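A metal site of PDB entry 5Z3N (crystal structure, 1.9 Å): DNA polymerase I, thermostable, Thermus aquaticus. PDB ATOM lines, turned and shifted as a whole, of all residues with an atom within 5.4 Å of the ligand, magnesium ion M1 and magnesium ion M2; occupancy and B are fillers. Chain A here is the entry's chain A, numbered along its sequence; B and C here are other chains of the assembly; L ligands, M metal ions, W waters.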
ATOM      1  N   ARG A 280      14.758 -11.109   4.210  1.00  0.00           N
ATOM      2  CA  ARG A 280      15.192 -10.529   5.468  1.00  0.00           C
ATOM      3  C   ARG A 280      14.203 -10.829   6.585  1.00  0.00           C
ATOM      4  O   ARG A 280      13.023 -11.066   6.354  1.00  0.00           O
ATOM      5  CB  ARG A 280      15.278  -9.036   5.326  1.00  0.00           C
ATOM      6  CG  ARG A 280      16.547  -8.577   4.671  1.00  0.00           C
ATOM      7  CD  ARG A 280      16.564  -7.072   4.812  1.00  0.00           C
ATOM      8  NE  ARG A 280      17.845  -6.524   4.462  1.00  0.00           N
ATOM      9  CZ  ARG A 280      18.155  -5.249   4.588  1.00  0.00           C
ATOM     10  NH1 ARG A 280      17.246  -4.372   5.024  1.00  0.00           N
ATOM     11  NH2 ARG A 280      19.385  -4.848   4.268  1.00  0.00           N
ATOM     12  N   ASP A 317      29.346  -7.094  12.412  1.00  0.00           N
ATOM     13  CA  ASP A 317      28.698  -6.499  11.243  1.00  0.00           C
ATOM     14  C   ASP A 317      29.484  -6.861   9.998  1.00  0.00           C
ATOM     15  O   ASP A 317      30.677  -6.578   9.927  1.00  0.00           O
ATOM     16  CB  ASP A 317      28.667  -4.962  11.401  1.00  0.00           C
ATOM     17  CG  ASP A 317      27.810  -4.293  10.365  1.00  0.00           C
ATOM     18  OD1 ASP A 317      28.004  -4.541   9.157  1.00  0.00           O
ATOM     19  OD2 ASP A 317      26.940  -3.473  10.759  1.00  0.00           O
ATOM     20  N   TYR A 318      28.827  -7.488   9.027  1.00  0.00           N
ATOM     21  CA  TYR A 318      29.490  -7.835   7.773  1.00  0.00           C
ATOM     22  C   TYR A 318      29.920  -6.582   7.021  1.00  0.00           C
ATOM     23  O   TYR A 318      29.161  -5.610   6.923  1.00  0.00           O
ATOM     24  CB  TYR A 318      28.582  -8.640   6.869  1.00  0.00           C
ATOM     25  CG  TYR A 318      28.432 -10.101   7.194  1.00  0.00           C
ATOM     26  CD1 TYR A 318      29.444 -11.008   6.869  1.00  0.00           C
ATOM     27  CD2 TYR A 318      27.255 -10.608   7.738  1.00  0.00           C
ATOM     28  CE1 TYR A 318      29.309 -12.376   7.122  1.00  0.00           C
ATOM     29  CE2 TYR A 318      27.099 -11.965   7.990  1.00  0.00           C
ATOM     30  CZ  TYR A 318      28.152 -12.841   7.686  1.00  0.00           C
ATOM     31  OH  TYR A 318      28.015 -14.174   7.910  1.00  0.00           O
ATOM     32  N   SER A 319      31.137  -6.598   6.527  1.00  0.00           N
ATOM     33  CA  SER A 319      31.726  -5.512   5.750  1.00  0.00           C
ATOM     34  C   SER A 319      31.173  -5.469   4.317  1.00  0.00           C
ATOM     35  O   SER A 319      31.310  -6.417   3.577  1.00  0.00           O
ATOM     36  CB  SER A 319      33.242  -5.701   5.695  1.00  0.00           C
ATOM     37  OG  SER A 319      33.851  -4.891   4.722  1.00  0.00           O
ATOM     38  N   GLN A 320      30.582  -4.343   3.899  1.00  0.00           N
ATOM     39  CA  GLN A 320      30.217  -4.115   2.504  1.00  0.00           C
ATOM     40  C   GLN A 320      29.450  -5.277   1.885  1.00  0.00           C
ATOM     41  O   GLN A 320      29.705  -5.671   0.729  1.00  0.00           O
ATOM     42  CB  GLN A 320      31.461  -3.871   1.668  1.00  0.00           C
ATOM     43  CG  GLN A 320      32.334  -2.742   2.184  1.00  0.00           C
ATOM     44  CD  GLN A 320      33.616  -2.629   1.409  1.00  0.00           C
ATOM     45  OE1 GLN A 320      33.636  -2.058   0.331  1.00  0.00           O
ATOM     46  NE2 GLN A 320      34.681  -3.193   1.943  1.00  0.00           N
ATOM     47  N   ILE A 321      28.511  -5.789   2.637  1.00  0.00           N
ATOM     48  CA  ILE A 321      28.011  -7.121   2.368  1.00  0.00           C
ATOM     49  C   ILE A 321      27.327  -7.300   1.012  1.00  0.00           C
ATOM     50  O   ILE A 321      27.703  -8.216   0.280  1.00  0.00           O
ATOM     51  CB  ILE A 321      27.155  -7.682   3.542  1.00  0.00           C
ATOM     52  CG1 ILE A 321      26.840  -9.160   3.314  1.00  0.00           C
ATOM     53  CG2 ILE A 321      25.838  -6.978   3.724  1.00  0.00           C
ATOM     54  CD1 ILE A 321      28.062 -10.047   3.223  1.00  0.00           C
ATOM     55  N   GLU A 322      26.364  -6.442   0.644  1.00  0.00           N
ATOM     56  CA  GLU A 322      25.700  -6.610  -0.655  1.00  0.00           C
ATOM     57  C   GLU A 322      26.663  -6.416  -1.856  1.00  0.00           C
ATOM     58  O   GLU A 322      26.449  -7.024  -2.878  1.00  0.00           O
ATOM     59  CB  GLU A 322      24.419  -5.774  -0.762  1.00  0.00           C
ATOM     60  CG  GLU A 322      23.302  -6.392   0.078  1.00  0.00           C
ATOM     61  CD  GLU A 322      21.977  -5.660   0.039  1.00  0.00           C
ATOM     62  OE1 GLU A 322      21.668  -4.990  -0.964  1.00  0.00           O
ATOM     63  OE2 GLU A 322      21.252  -5.753   1.035  1.00  0.00           O
ATOM     64  N   LEU A 323      27.738  -5.652  -1.682  1.00  0.00           N
ATOM     65  CA  LEU A 323      28.736  -5.494  -2.743  1.00  0.00           C
ATOM     66  C   LEU A 323      29.563  -6.767  -2.952  1.00  0.00           C
ATOM     67  O   LEU A 323      29.907  -7.095  -4.090  1.00  0.00           O
ATOM     68  CB  LEU A 323      29.651  -4.274  -2.519  1.00  0.00           C
ATOM     69  CG  LEU A 323      28.950  -2.899  -2.492  1.00  0.00           C
ATOM     70  CD1 LEU A 323      29.960  -1.775  -2.264  1.00  0.00           C
ATOM     71  CD2 LEU A 323      28.183  -2.642  -3.789  1.00  0.00           C
ATOM     72  N   ASP A 344      38.056  -0.964   0.407  1.00  0.00           N
ATOM     73  CA  ASP A 344      36.763  -0.508   0.893  1.00  0.00           C
ATOM     74  C   ASP A 344      36.154   0.520  -0.066  1.00  0.00           C
ATOM     75  O   ASP A 344      36.644   1.635  -0.189  1.00  0.00           O
ATOM     76  CB  ASP A 344      36.875   0.080   2.294  1.00  0.00           C
ATOM     77  CG  ASP A 344      35.553   0.217   2.976  1.00  0.00           C
ATOM     78  OD1 ASP A 344      34.596   0.746   2.352  1.00  0.00           O
ATOM     79  OD2 ASP A 344      35.441  -0.173   4.149  1.00  0.00           O
ATOM     80  N   HIS A 346      33.057   1.900   0.109  1.00  0.00           N
ATOM     81  CA  HIS A 346      32.371   2.998   0.804  1.00  0.00           C
ATOM     82  C   HIS A 346      33.352   4.105   1.168  1.00  0.00           C
ATOM     83  O   HIS A 346      33.069   5.283   0.940  1.00  0.00           O
ATOM     84  CB  HIS A 346      31.640   2.510   2.071  1.00  0.00           C
ATOM     85  CG  HIS A 346      30.597   1.478   1.803  1.00  0.00           C
ATOM     86  ND1 HIS A 346      29.804   1.477   0.663  1.00  0.00           N
ATOM     87  CD2 HIS A 346      30.192   0.407   2.523  1.00  0.00           C
ATOM     88  CE1 HIS A 346      28.987   0.446   0.688  1.00  0.00           C
ATOM     89  NE2 HIS A 346      29.198  -0.218   1.808  1.00  0.00           N
ATOM     90  N   ARG A 366      30.783   8.085   5.567  1.00  0.00           N
ATOM     91  CA  ARG A 366      30.666   6.711   5.121  1.00  0.00           C
ATOM     92  C   ARG A 366      29.194   6.363   4.867  1.00  0.00           C
ATOM     93  O   ARG A 366      28.902   5.744   3.874  1.00  0.00           O
ATOM     94  CB  ARG A 366      31.305   5.713   6.132  1.00  0.00           C
ATOM     95  CG  ARG A 366      31.319   4.277   5.638  1.00  0.00           C
ATOM     96  CD  ARG A 366      31.571   3.220   6.747  1.00  0.00           C
ATOM     97  NE  ARG A 366      31.611   1.846   6.209  1.00  0.00           N
ATOM     98  CZ  ARG A 366      32.595   1.385   5.454  1.00  0.00           C
ATOM     99  NH1 ARG A 366      32.565   0.146   5.004  1.00  0.00           N
ATOM    100  NH2 ARG A 366      33.627   2.155   5.122  1.00  0.00           N
ATOM    101  N   ARG A 367      28.288   6.810   5.743  1.00  0.00           N
ATOM    102  CA  ARG A 367      26.838   6.586   5.519  1.00  0.00           C
ATOM    103  C   ARG A 367      26.349   7.312   4.256  1.00  0.00           C
ATOM    104  O   ARG A 367      25.574   6.772   3.461  1.00  0.00           O
ATOM    105  CB  ARG A 367      26.030   6.976   6.768  1.00  0.00           C
ATOM    106  CG  ARG A 367      24.497   6.759   6.710  1.00  0.00           C
ATOM    107  CD  ARG A 367      24.022   5.334   6.321  1.00  0.00           C
ATOM    108  NE  ARG A 367      23.685   5.253   4.905  1.00  0.00           N
ATOM    109  CZ  ARG A 367      23.079   4.244   4.285  1.00  0.00           C
ATOM    110  NH1 ARG A 367      22.798   4.381   2.979  1.00  0.00           N
ATOM    111  NH2 ARG A 367      22.721   3.121   4.918  1.00  0.00           N
ATOM    112  N   LYS A 370      27.450   5.259   1.343  1.00  0.00           N
ATOM    113  CA  LYS A 370      26.600   4.072   1.179  1.00  0.00           C
ATOM    114  C   LYS A 370      25.377   4.355   0.308  1.00  0.00           C
ATOM    115  O   LYS A 370      25.005   3.548  -0.577  1.00  0.00           O
ATOM    116  CB  LYS A 370      26.153   3.527   2.544  1.00  0.00           C
ATOM    117  CG  LYS A 370      27.214   2.710   3.240  1.00  0.00           C
ATOM    118  CD  LYS A 370      26.716   2.182   4.582  1.00  0.00           C
ATOM    119  CE  LYS A 370      27.835   1.546   5.370  1.00  0.00           C
ATOM    120  NZ  LYS A 370      27.405   1.231   6.759  1.00  0.00           N
ATOM    121  N   THR A 371      24.755   5.502   0.543  1.00  0.00           N
ATOM    122  CA  THR A 371      23.613   5.933  -0.248  1.00  0.00           C
ATOM    123  C   THR A 371      23.963   6.012  -1.722  1.00  0.00           C
ATOM    124  O   THR A 371      23.196   5.542  -2.569  1.00  0.00           O
ATOM    125  CB  THR A 371      23.060   7.260   0.276  1.00  0.00           C
ATOM    126  OG1 THR A 371      22.641   7.063   1.636  1.00  0.00           O
ATOM    127  CG2 THR A 371      21.886   7.732  -0.543  1.00  0.00           C
ATOM    128  N   PHE A 374      24.967   2.137  -3.136  1.00  0.00           N
ATOM    129  CA  PHE A 374      23.795   1.285  -3.331  1.00  0.00           C
ATOM    130  C   PHE A 374      22.760   1.950  -4.234  1.00  0.00           C
ATOM    131  O   PHE A 374      22.187   1.285  -5.083  1.00  0.00           O
ATOM    132  CB  PHE A 374      23.209   0.841  -1.997  1.00  0.00           C
ATOM    133  CG  PHE A 374      24.181   0.019  -1.187  1.00  0.00           C
ATOM    134  CD1 PHE A 374      24.724  -1.143  -1.712  1.00  0.00           C
ATOM    135  CD2 PHE A 374      24.579   0.412   0.090  1.00  0.00           C
ATOM    136  CE1 PHE A 374      25.638  -1.911  -0.990  1.00  0.00           C
ATOM    137  CE2 PHE A 374      25.491  -0.352   0.821  1.00  0.00           C
ATOM    138  CZ  PHE A 374      26.010  -1.516   0.279  1.00  0.00           C
ATOM    139  N   GLY A 375      22.563   3.259  -4.054  1.00  0.00           N
ATOM    140  CA  GLY A 375      21.756   4.071  -4.959  1.00  0.00           C
ATOM    141  C   GLY A 375      22.097   3.844  -6.407  1.00  0.00           C
ATOM    142  O   GLY A 375      21.248   3.407  -7.179  1.00  0.00           O
ATOM    143  N   TYR A 378      21.440   0.099  -7.564  1.00  0.00           N
ATOM    144  CA  TYR A 378      20.039  -0.301  -7.658  1.00  0.00           C
ATOM    145  C   TYR A 378      19.149   0.664  -8.476  1.00  0.00           C
ATOM    146  O   TYR A 378      17.922   0.561  -8.419  1.00  0.00           O
ATOM    147  CB  TYR A 378      19.471  -0.545  -6.263  1.00  0.00           C
ATOM    148  CG  TYR A 378      20.167  -1.692  -5.554  1.00  0.00           C
ATOM    149  CD1 TYR A 378      20.247  -2.955  -6.143  1.00  0.00           C
ATOM    150  CD2 TYR A 378      20.746  -1.512  -4.308  1.00  0.00           C
ATOM    151  CE1 TYR A 378      20.872  -4.013  -5.518  1.00  0.00           C
ATOM    152  CE2 TYR A 378      21.361  -2.554  -3.649  1.00  0.00           C
ATOM    153  CZ  TYR A 378      21.435  -3.811  -4.265  1.00  0.00           C
ATOM    154  OH  TYR A 378      22.058  -4.864  -3.609  1.00  0.00           O
ATOM    155  N   ASN A 457      17.198  -6.233  -7.216  1.00  0.00           N
ATOM    156  CA  ASN A 457      17.677  -6.028  -5.863  1.00  0.00           C
ATOM    157  C   ASN A 457      17.554  -7.286  -5.021  1.00  0.00           C
ATOM    158  O   ASN A 457      18.419  -7.556  -4.167  1.00  0.00           O
ATOM    159  CB  ASN A 457      16.930  -4.883  -5.196  1.00  0.00           C
ATOM    160  CG  ASN A 457      17.225  -4.774  -3.714  1.00  0.00           C
ATOM    161  OD1 ASN A 457      16.554  -5.375  -2.890  1.00  0.00           O
ATOM    162  ND2 ASN A 457      18.267  -4.056  -3.381  1.00  0.00           N
ATOM    163  N   VAL A 490      20.351  -7.447  13.039  1.00  0.00           N
ATOM    164  CA  VAL A 490      20.059  -6.172  12.354  1.00  0.00           C
ATOM    165  C   VAL A 490      20.590  -6.302  10.916  1.00  0.00           C
ATOM    166  O   VAL A 490      21.417  -5.515  10.461  1.00  0.00           O
ATOM    167  CB  VAL A 490      20.615  -4.885  13.059  1.00  0.00           C
ATOM    168  CG1 VAL A 490      19.991  -3.607  12.481  1.00  0.00           C
ATOM    169  CG2 VAL A 490      20.364  -4.929  14.556  1.00  0.00           C
ATOM    170  N   ASP A 492      22.608  -7.475   8.693  1.00  0.00           N
ATOM    171  CA  ASP A 492      23.928  -8.050   8.486  1.00  0.00           C
ATOM    172  C   ASP A 492      24.779  -7.951   9.746  1.00  0.00           C
ATOM    173  O   ASP A 492      26.002  -8.029   9.680  1.00  0.00           O
ATOM    174  CB  ASP A 492      24.649  -7.372   7.321  1.00  0.00           C
ATOM    175  CG  ASP A 492      25.184  -6.015   7.669  1.00  0.00           C
ATOM    176  OD1 ASP A 492      24.576  -5.316   8.514  1.00  0.00           O
ATOM    177  OD2 ASP A 492      26.245  -5.637   7.129  1.00  0.00           O
ATOM    178  N   GLU A 493      24.108  -7.804  10.885  1.00  0.00           N
ATOM    179  CA  GLU A 493      24.754  -7.595  12.160  1.00  0.00           C
ATOM    180  C   GLU A 493      24.100  -8.475  13.186  1.00  0.00           C
ATOM    181  O   GLU A 493      22.878  -8.638  13.193  1.00  0.00           O
ATOM    182  CB  GLU A 493      24.625  -6.109  12.585  1.00  0.00           C
ATOM    183  CG  GLU A 493      25.033  -5.785  14.023  1.00  0.00           C
ATOM    184  CD  GLU A 493      24.752  -4.344  14.449  1.00  0.00           C
ATOM    185  OE1 GLU A 493      24.179  -3.572  13.663  1.00  0.00           O
ATOM    186  OE2 GLU A 493      25.156  -4.003  15.581  1.00  0.00           O
ATOM    187  N   LYS A 538      30.481  -1.097  18.578  1.00  0.00           N
ATOM    188  CA  LYS A 538      30.781  -0.981  17.130  1.00  0.00           C
ATOM    189  C   LYS A 538      31.893   0.001  16.826  1.00  0.00           C
ATOM    190  O   LYS A 538      32.139   0.294  15.657  1.00  0.00           O
ATOM    191  CB  LYS A 538      29.538  -0.546  16.376  1.00  0.00           C
ATOM    192  CG  LYS A 538      28.399  -1.539  16.506  1.00  0.00           C
ATOM    193  CD  LYS A 538      27.377  -1.412  15.389  1.00  0.00           C
ATOM    194  CE  LYS A 538      27.843  -2.019  14.084  1.00  0.00           C
ATOM    195  NZ  LYS A 538      26.735  -1.919  13.068  1.00  0.00           N
ATOM    196  P    DC B   4      15.537   7.629  -7.901  1.00  0.00           P
ATOM    197  OP1  DC B   4      14.952   8.190  -6.655  1.00  0.00           O
ATOM    198  OP2  DC B   4      16.396   8.461  -8.766  1.00  0.00           O
ATOM    199  O5'  DC B   4      16.305   6.338  -7.378  1.00  0.00           O
ATOM    200  C5'  DC B   4      15.646   5.403  -6.509  1.00  0.00           C
ATOM    201  C4'  DC B   4      16.339   4.071  -6.570  1.00  0.00           C
ATOM    202  O4'  DC B   4      17.714   4.210  -6.134  1.00  0.00           O
ATOM    203  C3'  DC B   4      15.741   2.987  -5.695  1.00  0.00           C
ATOM    204  O3'  DC B   4      14.668   2.354  -6.373  1.00  0.00           O
ATOM    205  C2'  DC B   4      16.929   2.085  -5.435  1.00  0.00           C
ATOM    206  C1'  DC B   4      18.082   3.092  -5.328  1.00  0.00           C
ATOM    207  N1   DC B   4      18.367   3.578  -3.956  1.00  0.00           N
ATOM    208  C2   DC B   4      18.949   2.684  -3.044  1.00  0.00           C
ATOM    209  O2   DC B   4      19.187   1.525  -3.407  1.00  0.00           O
ATOM    210  N3   DC B   4      19.225   3.107  -1.793  1.00  0.00           N
ATOM    211  C4   DC B   4      18.936   4.367  -1.434  1.00  0.00           C
ATOM    212  N4   DC B   4      19.214   4.737  -0.181  1.00  0.00           N
ATOM    213  C5   DC B   4      18.314   5.282  -2.333  1.00  0.00           C
ATOM    214  C6   DC B   4      18.074   4.846  -3.579  1.00  0.00           C
ATOM    215  P    DG B   5      13.313   1.970  -5.596  1.00  0.00           P
ATOM    216  OP1  DG B   5      12.327   1.549  -6.608  1.00  0.00           O
ATOM    217  OP2  DG B   5      13.002   3.033  -4.639  1.00  0.00           O
ATOM    218  O5'  DG B   5      13.718   0.668  -4.785  1.00  0.00           O
ATOM    219  C5'  DG B   5      13.981  -0.563  -5.450  1.00  0.00           C
ATOM    220  C4'  DG B   5      14.507  -1.579  -4.463  1.00  0.00           C
ATOM    221  O4'  DG B   5      15.723  -1.062  -3.884  1.00  0.00           O
ATOM    222  C3'  DG B   5      13.607  -1.860  -3.272  1.00  0.00           C
ATOM    223  O3'  DG B   5      12.708  -2.920  -3.554  1.00  0.00           O
ATOM    224  C2'  DG B   5      14.603  -2.309  -2.218  1.00  0.00           C
ATOM    225  C1'  DG B   5      15.829  -1.483  -2.542  1.00  0.00           C
ATOM    226  N9   DG B   5      16.012  -0.305  -1.701  1.00  0.00           N
ATOM    227  C8   DG B   5      15.756   1.019  -1.978  1.00  0.00           C
ATOM    228  N7   DG B   5      16.075   1.819  -1.003  1.00  0.00           N
ATOM    229  C5   DG B   5      16.567   0.967  -0.011  1.00  0.00           C
ATOM    230  C6   DG B   5      17.064   1.262   1.284  1.00  0.00           C
ATOM    231  O6   DG B   5      17.194   2.355   1.830  1.00  0.00           O
ATOM    232  N1   DG B   5      17.425   0.094   1.963  1.00  0.00           N
ATOM    233  C2   DG B   5      17.324  -1.171   1.448  1.00  0.00           C
ATOM    234  N2   DG B   5      17.744  -2.174   2.238  1.00  0.00           N
ATOM    235  N3   DG B   5      16.874  -1.455   0.242  1.00  0.00           N
ATOM    236  C4   DG B   5      16.512  -0.337  -0.426  1.00  0.00           C
ATOM    237  N1  DOC C  12      19.709  -0.702   6.385  1.00  0.00           N
ATOM    238  C2  DOC C  12      19.037  -0.787   5.171  1.00  0.00           C
ATOM    239  N3  DOC C  12      18.812   0.313   4.472  1.00  0.00           N
ATOM    240  C4  DOC C  12      19.206   1.512   4.897  1.00  0.00           C
ATOM    241  C5  DOC C  12      19.877   1.614   6.092  1.00  0.00           C
ATOM    242  C6  DOC C  12      20.129   0.445   6.808  1.00  0.00           C
ATOM    243  O2  DOC C  12      18.645  -1.868   4.772  1.00  0.00           O
ATOM    244  N4  DOC C  12      18.972   2.588   4.172  1.00  0.00           N
ATOM    245  C1' DOC C  12      19.932  -1.946   7.150  1.00  0.00           C
ATOM    246  C2' DOC C  12      21.244  -2.623   6.760  1.00  0.00           C
ATOM    247  C3' DOC C  12      22.166  -2.195   7.854  1.00  0.00           C
ATOM    248  C4' DOC C  12      21.188  -2.068   9.016  1.00  0.00           C
ATOM    249  O4' DOC C  12      19.975  -1.673   8.506  1.00  0.00           O
ATOM    250  C5' DOC C  12      21.654  -1.103  10.129  1.00  0.00           C
ATOM    251  O5' DOC C  12      21.863   0.218   9.681  1.00  0.00           O
ATOM    252  P   DOC C  12      22.378   1.291  10.643  1.00  0.00           P
ATOM    253  OP1 DOC C  12      23.387   0.777  11.525  1.00  0.00           O
ATOM    254  OP2 DOC C  12      22.644   2.429   9.886  1.00  0.00           O
HETATM  255  P1  LIG L   1      29.754  -1.679   6.369  1.00  0.00           P
HETATM  256  O1  LIG L   1      29.047  -2.665   7.258  1.00  0.00           O
HETATM  257  O2  LIG L   1      29.727  -0.259   6.855  1.00  0.00           O
HETATM  258  O3  LIG L   1      31.084  -2.121   5.841  1.00  0.00           O
HETATM  259  O4  LIG L   1      28.867  -1.619   5.002  1.00  0.00           O
HETATM  260  P2  LIG L   1      27.593  -2.486   4.545  1.00  0.00           P
HETATM  261  O5  LIG L   1      27.555  -2.354   3.061  1.00  0.00           O
HETATM  262  O6  LIG L   1      27.550  -3.891   5.081  1.00  0.00           O
HETATM  263  O7  LIG L   1      26.399  -1.552   5.113  1.00  0.00           O
HETATM  264  P3  LIG L   1      25.436  -1.827   6.363  1.00  0.00           P
HETATM  265  O8  LIG L   1      25.052  -0.508   6.917  1.00  0.00           O
HETATM  266  O9  LIG L   1      26.083  -2.771   7.339  1.00  0.00           O
HETATM  267  O10 LIG L   1      24.143  -2.451   5.651  1.00  0.00           O
HETATM  268  C1  LIG L   1      24.046  -3.814   5.262  1.00  0.00           C
HETATM  269  C2  LIG L   1      23.452  -3.951   3.867  1.00  0.00           C
HETATM  270  O11 LIG L   1      22.094  -3.477   3.824  1.00  0.00           O
HETATM  271  C3  LIG L   1      24.217  -3.191   2.791  1.00  0.00           C
HETATM  272  O12 LIG L   1      25.305  -3.946   2.247  1.00  0.00           O
HETATM  273  C4  LIG L   1      23.152  -2.948   1.767  1.00  0.00           C
HETATM  274  C5  LIG L   1      21.869  -2.805   2.583  1.00  0.00           C
HETATM  275  N1  LIG L   1      21.739  -1.338   2.687  1.00  0.00           N
HETATM  276  C6  LIG L   1      22.202  -0.499   3.640  1.00  0.00           C
HETATM  277  N2  LIG L   1      21.932   0.789   3.308  1.00  0.00           N
HETATM  278  C7  LIG L   1      21.315   0.767   2.126  1.00  0.00           C
HETATM  279  C8  LIG L   1      20.770   1.759   1.168  1.00  0.00           C
HETATM  280  O13 LIG L   1      20.833   2.975   1.444  1.00  0.00           O
HETATM  281  N3  LIG L   1      20.199   1.306   0.039  1.00  0.00           N
HETATM  282  C9  LIG L   1      20.143  -0.006  -0.281  1.00  0.00           C
HETATM  283  N4  LIG L   1      19.575  -0.414  -1.430  1.00  0.00           N
HETATM  284  N5  LIG L   1      20.622  -0.969   0.542  1.00  0.00           N
HETATM  285  C10 LIG L   1      21.201  -0.626   1.712  1.00  0.00           C
HETATM  286 MG    MG M   1      27.665  -4.195   7.066  1.00  0.00          MG
HETATM  287 MG    MG M   2      25.081  -3.407   9.428  1.00  0.00          MG
HETATM  288  O   HOH W   1      23.441  -3.666  11.045  1.00  0.00           O
HETATM  289  O   HOH W   2      30.966  -3.883   8.980  1.00  0.00           O
HETATM  290  O   HOH W   3      33.301  -2.611   7.575  1.00  0.00           O
HETATM  291  O   HOH W   4      21.624  -6.824   3.540  1.00  0.00           O
HETATM  292  O   HOH W   5      23.808   1.887   7.135  1.00  0.00           O
HETATM  293  O   HOH W   6      19.358  -3.662  -0.491  1.00  0.00           O
HETATM  294  O   HOH W   7      24.991  -0.799   9.768  1.00  0.00           O
HETATM  295  O   HOH W   8      28.010  -0.901   9.446  1.00  0.00           O
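Of the 25 residues printed, 3 come within 4 Å of magnesium ion M1.
The side-chain amino group (NZ) of Lys 538 lies close to the side-chain carboxylate (OD2) of Asp 317 (2.8 Å). NH1 of Arg 367 is in hydrogen-bond range of OG1 of Thr 371 (3.0 Å). O2 of DOC 12 of chain C lies within hydrogen-bond range of the guanidinium group (NH1) of Arg 280, 2.9 Å away. N2 of DG 5 of chain B lies close to O2 of DOC 12 of chain C. The backbone NH (N) of His 346 sits at hydrogen-bond distance from the side-chain carboxylate (OD1) of Asp 344, 3.0 Å away. The side-chain hydroxyl (OG) of Ser 319 lies within hydrogen-bond range of the side-chain amide nitrogen (NE2) of Gln 320, at 3.4 Å. The guanidinium group (NH2) of Arg 280 lies within salt-bridge range of the side-chain carboxylate (OE2) of Glu 322, 3.8 Å away. The side-chain hydroxyl (OH) of Tyr 378 is in hydrogen-bond range of the side-chain carboxylate (OE1) of Glu 322 (2.7 Å).
N3 of DC 4 of chain B sits at hydrogen-bond distance from a nitrogen (N3) of the ligand. O2 of the ligand lies within salt-bridge range of NZ of Lys 370 (2.8 Å). The guanidinium group (NH1) of Arg 366 lies within salt-bridge range of an oxygen (O3) of the ligand, 2.8 Å away. The guanidinium group of Arg 367 is in hydrogen-bond range of an oxygen (O13) of the ligand. O5 of the ligand sits at hydrogen-bond distance from NE2 of His 346, 3.0 Å away. N of Gln 320 sits at hydrogen-bond distance from O3 of the ligand, 3.0 Å away. NH2 of Arg 280 lies within hydrogen-bond range of O11 of the ligand (3.1 Å). An oxygen (O12) of the ligand is in hydrogen-bond range of the backbone NH (N) of Glu 322 (3.1 Å). A nitrogen (N4) of the ligand sits close to N3 of DG 5 of chain B (3.3 Å). An oxygen (O6) of the ligand sits close to the backbone NH (N) of Ile 321, 3.2 Å away.
Residues that only touch magnesium ion M2: DOC 12 of chain C (3.5 Å). Along chain A the residues within 4 Å of magnesium ion M2 span positions 317 to 492.
Magnesium ion M2 is bound by the side-chain carboxylate (OD1) of Asp 492, the side-chain carboxylate (OD2) of Asp 317, water W1 and an oxygen (O9) of the ligand. Magnesium ion M2 has four donor atoms within binding distance. Slightly farther from magnesium ion M2 lies water W7 (2.6 Å).
Water W1 lies within hydrogen-bond range of the side-chain carboxylate (OE1) of Glu 493 (2.7 Å) and the backbone carbonyl oxygen (O) of Val 490 (2.8 Å). Water W7 bridges OP1 of DOC 12 of chain C (2.9 Å) and O8 of the ligand (2.9 Å). Water W5 lies within hydrogen-bond range of an oxygen (O8) of the ligand (2.7 Å), the guanidinium group (NH2) of Arg 367 (2.8 Å) and OP2 of DOC 12 of chain C (3.0 Å). Water W8 lies within hydrogen-bond range of an oxygen (O2) of the ligand (3.2 Å) and the side-chain amino group (NZ) of Lys 370 (3.5 Å). Water W4 lies within hydrogen-bond range of OE2 of Glu 322 (2.7 Å), NH2 of Arg 280 (3.1 Å) and O11 of the ligand (3.4 Å).
Magnesium ion M1 is bound by O6 of the ligand (2.0 Å), OD2 of Asp 492 (2.0 Å), O of Tyr 318 (2.1 Å), O1 of the ligand (2.1 Å), O9 of the ligand (2.1 Å) and OD1 of Asp 317 (2.1 Å).
N4 of DOC 12 of chain C lies close to O13 of the ligand (3.3 Å). Residues that only touch the ligand: Ser 319 (3.5 Å), Phe 374 (3.2 Å) and Tyr 378 (3.3 Å). Hydrophobic or aromatic side chains that line the ligand: Ile 321, His 346, Phe 374 and Tyr 378. 17 residues have an atom within 4 Å of the ligand: Arg 280, Asp 317, Tyr 318, Ser 319, Gln 320, Ile 321, Glu 322, His 346, Arg 366, Arg 367, Lys 370, Phe 374, Tyr 378, Asp 492, DC 4 of chain B, DG 5 of chain B and DOC 12 of chain C. The nearest printed residue that does not touch the ligand is Asn 457 (4.3 Å).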
